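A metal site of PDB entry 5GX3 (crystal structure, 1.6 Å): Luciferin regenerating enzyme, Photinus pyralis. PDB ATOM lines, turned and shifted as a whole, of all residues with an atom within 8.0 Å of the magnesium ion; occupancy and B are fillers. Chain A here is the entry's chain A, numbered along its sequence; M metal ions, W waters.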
ATOM      1  N   VAL A  19      28.042  -7.581  27.383  1.00  0.00           N
ATOM      2  CA  VAL A  19      27.311  -8.844  27.284  1.00  0.00           C
ATOM      3  C   VAL A  19      26.132  -8.773  28.251  1.00  0.00           C
ATOM      4  O   VAL A  19      26.224  -9.235  29.393  1.00  0.00           O
ATOM      5  CB  VAL A  19      28.193 -10.063  27.582  1.00  0.00           C
ATOM      6  CG1 VAL A  19      27.404 -11.342  27.312  1.00  0.00           C
ATOM      7  CG2 VAL A  19      29.476 -10.069  26.741  1.00  0.00           C
ATOM      8  N   GLY A  20      25.039  -8.141  27.833  1.00  0.00           N
ATOM      9  CA  GLY A  20      23.821  -8.180  28.645  1.00  0.00           C
ATOM     10  C   GLY A  20      23.316  -9.613  28.732  1.00  0.00           C
ATOM     11  O   GLY A  20      23.392 -10.370  27.756  1.00  0.00           O
ATOM     12  N   GLU A  21      22.807  -9.996  29.902  1.00  0.00           N
ATOM     13  CA  GLU A  21      22.564 -11.401  30.213  1.00  0.00           C
ATOM     14  C   GLU A  21      21.633 -11.550  31.412  1.00  0.00           C
ATOM     15  O   GLU A  21      21.321 -10.584  32.118  1.00  0.00           O
ATOM     16  CB  GLU A  21      23.880 -12.154  30.496  1.00  0.00           C
ATOM     17  CG  GLU A  21      24.428 -12.936  29.307  1.00  0.00           C
ATOM     18  CD  GLU A  21      23.685 -14.247  29.076  1.00  0.00           C
ATOM     19  OE1 GLU A  21      24.195 -15.102  28.319  1.00  0.00           O
ATOM     20  OE2 GLU A  21      22.590 -14.427  29.657  1.00  0.00           O
ATOM     21  N   GLY A  22      21.210 -12.797  31.655  1.00  0.00           N
ATOM     22  CA  GLY A  22      20.503 -13.169  32.861  1.00  0.00           C
ATOM     23  C   GLY A  22      19.252 -12.367  33.216  1.00  0.00           C
ATOM     24  O   GLY A  22      19.043 -12.015  34.379  1.00  0.00           O
ATOM     25  N   PRO A  23      18.372 -12.108  32.255  1.00  0.00           N
ATOM     26  CA  PRO A  23      17.164 -11.336  32.575  1.00  0.00           C
ATOM     27  C   PRO A  23      16.234 -12.101  33.497  1.00  0.00           C
ATOM     28  O   PRO A  23      16.026 -13.306  33.354  1.00  0.00           O
ATOM     29  CB  PRO A  23      16.520 -11.100  31.212  1.00  0.00           C
ATOM     30  CG  PRO A  23      16.954 -12.291  30.406  1.00  0.00           C
ATOM     31  CD  PRO A  23      18.371 -12.552  30.842  1.00  0.00           C
ATOM     32  N   THR A  37      27.827  -9.864  31.912  1.00  0.00           N
ATOM     33  CA  THR A  37      28.722 -10.916  32.376  1.00  0.00           C
ATOM     34  C   THR A  37      30.197 -10.567  32.223  1.00  0.00           C
ATOM     35  O   THR A  37      31.033 -11.313  32.735  1.00  0.00           O
ATOM     36  CB  THR A  37      28.462 -12.250  31.661  1.00  0.00           C
ATOM     37  OG1 THR A  37      28.535 -12.078  30.243  1.00  0.00           O
ATOM     38  CG2 THR A  37      27.100 -12.795  32.019  1.00  0.00           C
ATOM     39  N   SER A  62      26.950 -13.359  36.763  1.00  0.00           N
ATOM     40  CA  SER A  62      26.212 -13.998  35.673  1.00  0.00           C
ATOM     41  C   SER A  62      24.714 -14.192  35.908  1.00  0.00           C
ATOM     42  O   SER A  62      24.017 -14.535  34.952  1.00  0.00           O
ATOM     43  CB  SER A  62      26.850 -15.353  35.344  1.00  0.00           C
ATOM     44  OG  SER A  62      26.785 -16.245  36.461  1.00  0.00           O
ATOM     45  N   ASN A 113      28.180 -19.324  35.230  1.00  0.00           N
ATOM     46  CA  ASN A 113      27.497 -18.665  34.121  1.00  0.00           C
ATOM     47  C   ASN A 113      25.984 -18.701  34.359  1.00  0.00           C
ATOM     48  O   ASN A 113      25.536 -18.253  35.415  1.00  0.00           O
ATOM     49  CB  ASN A 113      27.888 -19.273  32.765  1.00  0.00           C
ATOM     50  CG  ASN A 113      27.549 -18.344  31.606  1.00  0.00           C
ATOM     51  OD1 ASN A 113      27.435 -17.127  31.789  1.00  0.00           O
ATOM     52  ND2 ASN A 113      27.386 -18.903  30.406  1.00  0.00           N
ATOM     53  N   ASP A 114      25.166 -19.207  33.428  1.00  0.00           N
ATOM     54  CA  ASP A 114      23.733 -18.993  33.564  1.00  0.00           C
ATOM     55  C   ASP A 114      23.171 -19.725  34.782  1.00  0.00           C
ATOM     56  O   ASP A 114      23.664 -20.782  35.186  1.00  0.00           O
ATOM     57  CB  ASP A 114      23.001 -19.409  32.287  1.00  0.00           C
ATOM     58  CG  ASP A 114      21.757 -18.574  32.014  1.00  0.00           C
ATOM     59  OD1 ASP A 114      21.408 -17.695  32.848  1.00  0.00           O
ATOM     60  OD2 ASP A 114      21.090 -18.798  30.968  1.00  0.00           O
ATOM     61  N   GLY A 115      22.167 -19.120  35.398  1.00  0.00           N
ATOM     62  CA  GLY A 115      21.516 -19.706  36.573  1.00  0.00           C
ATOM     63  C   GLY A 115      20.064 -19.261  36.625  1.00  0.00           C
ATOM     64  O   GLY A 115      19.711 -18.174  36.144  1.00  0.00           O
ATOM     65  N   MET A 128      31.976 -22.707  33.771  1.00  0.00           N
ATOM     66  CA  MET A 128      32.708 -22.706  32.507  1.00  0.00           C
ATOM     67  C   MET A 128      34.088 -22.112  32.764  1.00  0.00           C
ATOM     68  O   MET A 128      34.295 -21.380  33.741  1.00  0.00           O
ATOM     69  CB  MET A 128      31.984 -21.884  31.438  1.00  0.00           C
ATOM     70  CG  MET A 128      31.907 -20.396  31.828  1.00  0.00           C
ATOM     71  SD  MET A 128      31.003 -19.292  30.716  1.00  0.00           S
ATOM     72  CE  MET A 128      32.242 -18.970  29.449  1.00  0.00           C
ATOM     73  N   ILE A 161      30.186 -24.290  27.806  1.00  0.00           N
ATOM     74  CA  ILE A 161      29.627 -22.991  28.183  1.00  0.00           C
ATOM     75  C   ILE A 161      28.250 -23.235  28.788  1.00  0.00           C
ATOM     76  O   ILE A 161      27.268 -23.453  28.068  1.00  0.00           O
ATOM     77  CB  ILE A 161      29.575 -22.010  27.017  1.00  0.00           C
ATOM     78  CG1 ILE A 161      30.997 -21.690  26.529  1.00  0.00           C
ATOM     79  CG2 ILE A 161      28.898 -20.704  27.452  1.00  0.00           C
ATOM     80  CD1 ILE A 161      31.067 -20.724  25.362  1.00  0.00           C
ATOM     81  N   ALA A 162      28.175 -23.213  30.129  1.00  0.00           N
ATOM     82  CA  ALA A 162      26.939 -23.508  30.853  1.00  0.00           C
ATOM     83  C   ALA A 162      25.885 -22.438  30.608  1.00  0.00           C
ATOM     84  O   ALA A 162      26.088 -21.267  30.958  1.00  0.00           O
ATOM     85  CB  ALA A 162      27.260 -23.604  32.347  1.00  0.00           C
ATOM     86  N   ASN A 163      24.749 -22.809  30.021  1.00  0.00           N
ATOM     87  CA  ASN A 163      23.819 -21.745  29.640  1.00  0.00           C
ATOM     88  C   ASN A 163      22.362 -22.042  30.004  1.00  0.00           C
ATOM     89  O   ASN A 163      22.100 -22.477  31.119  1.00  0.00           O
ATOM     90  CB  ASN A 163      24.038 -21.416  28.159  1.00  0.00           C
ATOM     91  CG  ASN A 163      24.687 -20.067  27.990  1.00  0.00           C
ATOM     92  OD1 ASN A 163      24.355 -19.143  28.724  1.00  0.00           O
ATOM     93  ND2 ASN A 163      25.634 -19.945  27.060  1.00  0.00           N
ATOM     94  N   GLY A 164      21.412 -21.767  29.104  1.00  0.00           N
ATOM     95  CA  GLY A 164      20.026 -21.580  29.523  1.00  0.00           C
ATOM     96  C   GLY A 164      19.358 -22.822  30.093  1.00  0.00           C
ATOM     97  O   GLY A 164      19.642 -23.958  29.707  1.00  0.00           O
ATOM     98  N   ILE A 177      21.116 -26.151  28.103  1.00  0.00           N
ATOM     99  CA  ILE A 177      21.945 -25.754  26.964  1.00  0.00           C
ATOM    100  C   ILE A 177      23.395 -25.659  27.401  1.00  0.00           C
ATOM    101  O   ILE A 177      23.735 -24.863  28.291  1.00  0.00           O
ATOM    102  CB  ILE A 177      21.487 -24.418  26.379  1.00  0.00           C
ATOM    103  CG1 ILE A 177      20.123 -24.543  25.700  1.00  0.00           C
ATOM    104  CG2 ILE A 177      22.538 -23.874  25.397  1.00  0.00           C
ATOM    105  CD1 ILE A 177      19.441 -23.196  25.503  1.00  0.00           C
ATOM    106  N   SER A 179      26.337 -24.305  25.234  1.00  0.00           N
ATOM    107  CA  SER A 179      26.406 -23.654  23.930  1.00  0.00           C
ATOM    108  C   SER A 179      27.324 -24.405  22.972  1.00  0.00           C
ATOM    109  O   SER A 179      27.054 -24.448  21.756  1.00  0.00           O
ATOM    110  CB  SER A 179      26.873 -22.214  24.079  1.00  0.00           C
ATOM    111  OG  SER A 179      25.930 -21.448  24.802  1.00  0.00           O
ATOM    112  N   PRO A 214      23.074 -21.793  20.718  1.00  0.00           N
ATOM    113  CA  PRO A 214      22.041 -21.546  21.724  1.00  0.00           C
ATOM    114  C   PRO A 214      22.668 -20.966  22.987  1.00  0.00           C
ATOM    115  O   PRO A 214      23.777 -21.337  23.371  1.00  0.00           O
ATOM    116  CB  PRO A 214      21.448 -22.932  21.975  1.00  0.00           C
ATOM    117  CG  PRO A 214      22.590 -23.870  21.700  1.00  0.00           C
ATOM    118  CD  PRO A 214      23.380 -23.230  20.568  1.00  0.00           C
ATOM    119  N   ASP A 215      21.964 -20.026  23.616  1.00  0.00           N
ATOM    120  CA  ASP A 215      22.506 -19.312  24.760  1.00  0.00           C
ATOM    121  C   ASP A 215      21.492 -19.431  25.894  1.00  0.00           C
ATOM    122  O   ASP A 215      21.313 -20.541  26.408  1.00  0.00           O
ATOM    123  CB  ASP A 215      22.844 -17.860  24.362  1.00  0.00           C
ATOM    124  CG  ASP A 215      23.820 -17.172  25.331  1.00  0.00           C
ATOM    125  OD1 ASP A 215      23.869 -17.536  26.520  1.00  0.00           O
ATOM    126  OD2 ASP A 215      24.545 -16.241  24.889  1.00  0.00           O
ATOM    127  N   GLY A 216      20.779 -18.359  26.262  1.00  0.00           N
ATOM    128  CA  GLY A 216      19.707 -18.476  27.238  1.00  0.00           C
ATOM    129  C   GLY A 216      18.424 -19.057  26.652  1.00  0.00           C
ATOM    130  O   GLY A 216      18.239 -19.082  25.434  1.00  0.00           O
ATOM    131  N   GLN A 217      17.531 -19.525  27.521  1.00  0.00           N
ATOM    132  CA  GLN A 217      16.219 -19.968  27.055  1.00  0.00           C
ATOM    133  C   GLN A 217      15.171 -19.770  28.146  1.00  0.00           C
ATOM    134  O   GLN A 217      15.496 -19.625  29.327  1.00  0.00           O
ATOM    135  CB  GLN A 217      16.224 -21.433  26.604  1.00  0.00           C
ATOM    136  CG  GLN A 217      16.507 -22.448  27.720  1.00  0.00           C
ATOM    137  CD  GLN A 217      16.455 -23.873  27.227  1.00  0.00           C
ATOM    138  OE1 GLN A 217      15.843 -24.168  26.188  1.00  0.00           O
ATOM    139  NE2 GLN A 217      17.121 -24.769  27.930  1.00  0.00           N
ATOM    140  N   ALA A 228      17.527 -18.093  22.786  1.00  0.00           N
ATOM    141  CA  ALA A 228      18.366 -17.042  22.239  1.00  0.00           C
ATOM    142  C   ALA A 228      19.480 -17.641  21.386  1.00  0.00           C
ATOM    143  O   ALA A 228      20.126 -18.605  21.793  1.00  0.00           O
ATOM    144  CB  ALA A 228      18.957 -16.212  23.375  1.00  0.00           C
ATOM    145  N   PHE A 230      22.949 -16.875  19.858  1.00  0.00           N
ATOM    146  CA  PHE A 230      24.133 -16.023  19.830  1.00  0.00           C
ATOM    147  C   PHE A 230      24.835 -16.201  18.486  1.00  0.00           C
ATOM    148  O   PHE A 230      25.156 -17.314  18.092  1.00  0.00           O
ATOM    149  CB  PHE A 230      25.046 -16.399  21.001  1.00  0.00           C
ATOM    150  CG  PHE A 230      26.199 -15.454  21.203  1.00  0.00           C
ATOM    151  CD1 PHE A 230      26.095 -14.394  22.086  1.00  0.00           C
ATOM    152  CD2 PHE A 230      27.393 -15.636  20.521  1.00  0.00           C
ATOM    153  CE1 PHE A 230      27.169 -13.515  22.280  1.00  0.00           C
ATOM    154  CE2 PHE A 230      28.462 -14.746  20.699  1.00  0.00           C
ATOM    155  CZ  PHE A 230      28.347 -13.696  21.566  1.00  0.00           C
ATOM    156  N   VAL A 257      22.413 -12.330  20.219  1.00  0.00           N
ATOM    157  CA  VAL A 257      21.310 -12.484  21.153  1.00  0.00           C
ATOM    158  C   VAL A 257      21.740 -13.427  22.271  1.00  0.00           C
ATOM    159  O   VAL A 257      22.266 -14.512  21.994  1.00  0.00           O
ATOM    160  CB  VAL A 257      20.070 -13.025  20.428  1.00  0.00           C
ATOM    161  CG1 VAL A 257      18.893 -13.150  21.382  1.00  0.00           C
ATOM    162  CG2 VAL A 257      19.723 -12.130  19.247  1.00  0.00           C
ATOM    163  N   THR A 258      21.534 -13.028  23.530  1.00  0.00           N
ATOM    164  CA  THR A 258      22.072 -13.779  24.674  1.00  0.00           C
ATOM    165  C   THR A 258      21.017 -14.457  25.535  1.00  0.00           C
ATOM    166  O   THR A 258      21.251 -15.575  25.982  1.00  0.00           O
ATOM    167  CB  THR A 258      22.911 -12.870  25.580  1.00  0.00           C
ATOM    168  OG1 THR A 258      22.104 -11.775  26.047  1.00  0.00           O
ATOM    169  CG2 THR A 258      24.120 -12.324  24.814  1.00  0.00           C
ATOM    170  N   SER A 259      19.883 -13.834  25.825  1.00  0.00           N
ATOM    171  CA  SER A 259      18.915 -14.499  26.692  1.00  0.00           C
ATOM    172  C   SER A 259      17.537 -13.863  26.525  1.00  0.00           C
ATOM    173  O   SER A 259      17.350 -12.896  25.775  1.00  0.00           O
ATOM    174  CB  SER A 259      19.363 -14.499  28.161  1.00  0.00           C
ATOM    175  OG  SER A 259      18.670 -15.526  28.868  1.00  0.00           O
ATOM    176  N   THR A 273      17.955  -9.861  25.783  1.00  0.00           N
ATOM    177  CA  THR A 273      19.260  -9.240  25.970  1.00  0.00           C
ATOM    178  C   THR A 273      20.196  -9.623  24.822  1.00  0.00           C
ATOM    179  O   THR A 273      19.988 -10.619  24.128  1.00  0.00           O
ATOM    180  CB  THR A 273      19.889  -9.651  27.301  1.00  0.00           C
ATOM    181  OG1 THR A 273      19.869 -11.078  27.408  1.00  0.00           O
ATOM    182  CG2 THR A 273      19.126  -9.048  28.497  1.00  0.00           C
HETATM  183 MG    MG M   1      24.237 -17.096  28.534  1.00  0.00          MG
HETATM  184  O   HOH W   1      22.286 -17.030  28.991  1.00  0.00           O
HETATM  185  O   HOH W   2      24.785 -16.815  30.617  1.00  0.00           O
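The magnesium ion is bound by water W1 (2.0 Å). The side-chain carboxylate (OE1) of Glu 21 binds the magnesium ion (2.0 Å). The side-chain amide oxygen (OD1) of Asn 163 binds the magnesium ion (2.1 Å). The magnesium ion is bound by OD1 of Asp 215 (2.1 Å). Water W2 is bound to the magnesium ion (2.2 Å).
Water W2 bridges the side-chain amide oxygen (OD1) of Asn 113 and the side-chain carboxylate (OE2) of Glu 21.
Within 4 Å of the magnesium ion: Glu 21, Asn 163 and Asp 215.
The backbone NH (N) of Gly 164 lies within hydrogen-bond range of the backbone carbonyl oxygen (O) of Asp 215, 3.0 Å away. N of Asp 215 lies within hydrogen-bond range of O of Ala 228 (3.0 Å). OG of Ser 179 sits at hydrogen-bond distance from ND2 of Asn 163 (2.7 Å). The backbone NH of Asn 163 sits at hydrogen-bond distance from the backbone carbonyl oxygen of Ile 177 (2.9 Å). The side-chain amide oxygen (OD1) of Asn 163 sits close to the side-chain amide nitrogen (ND2) of Asn 113 (3.5 Å).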
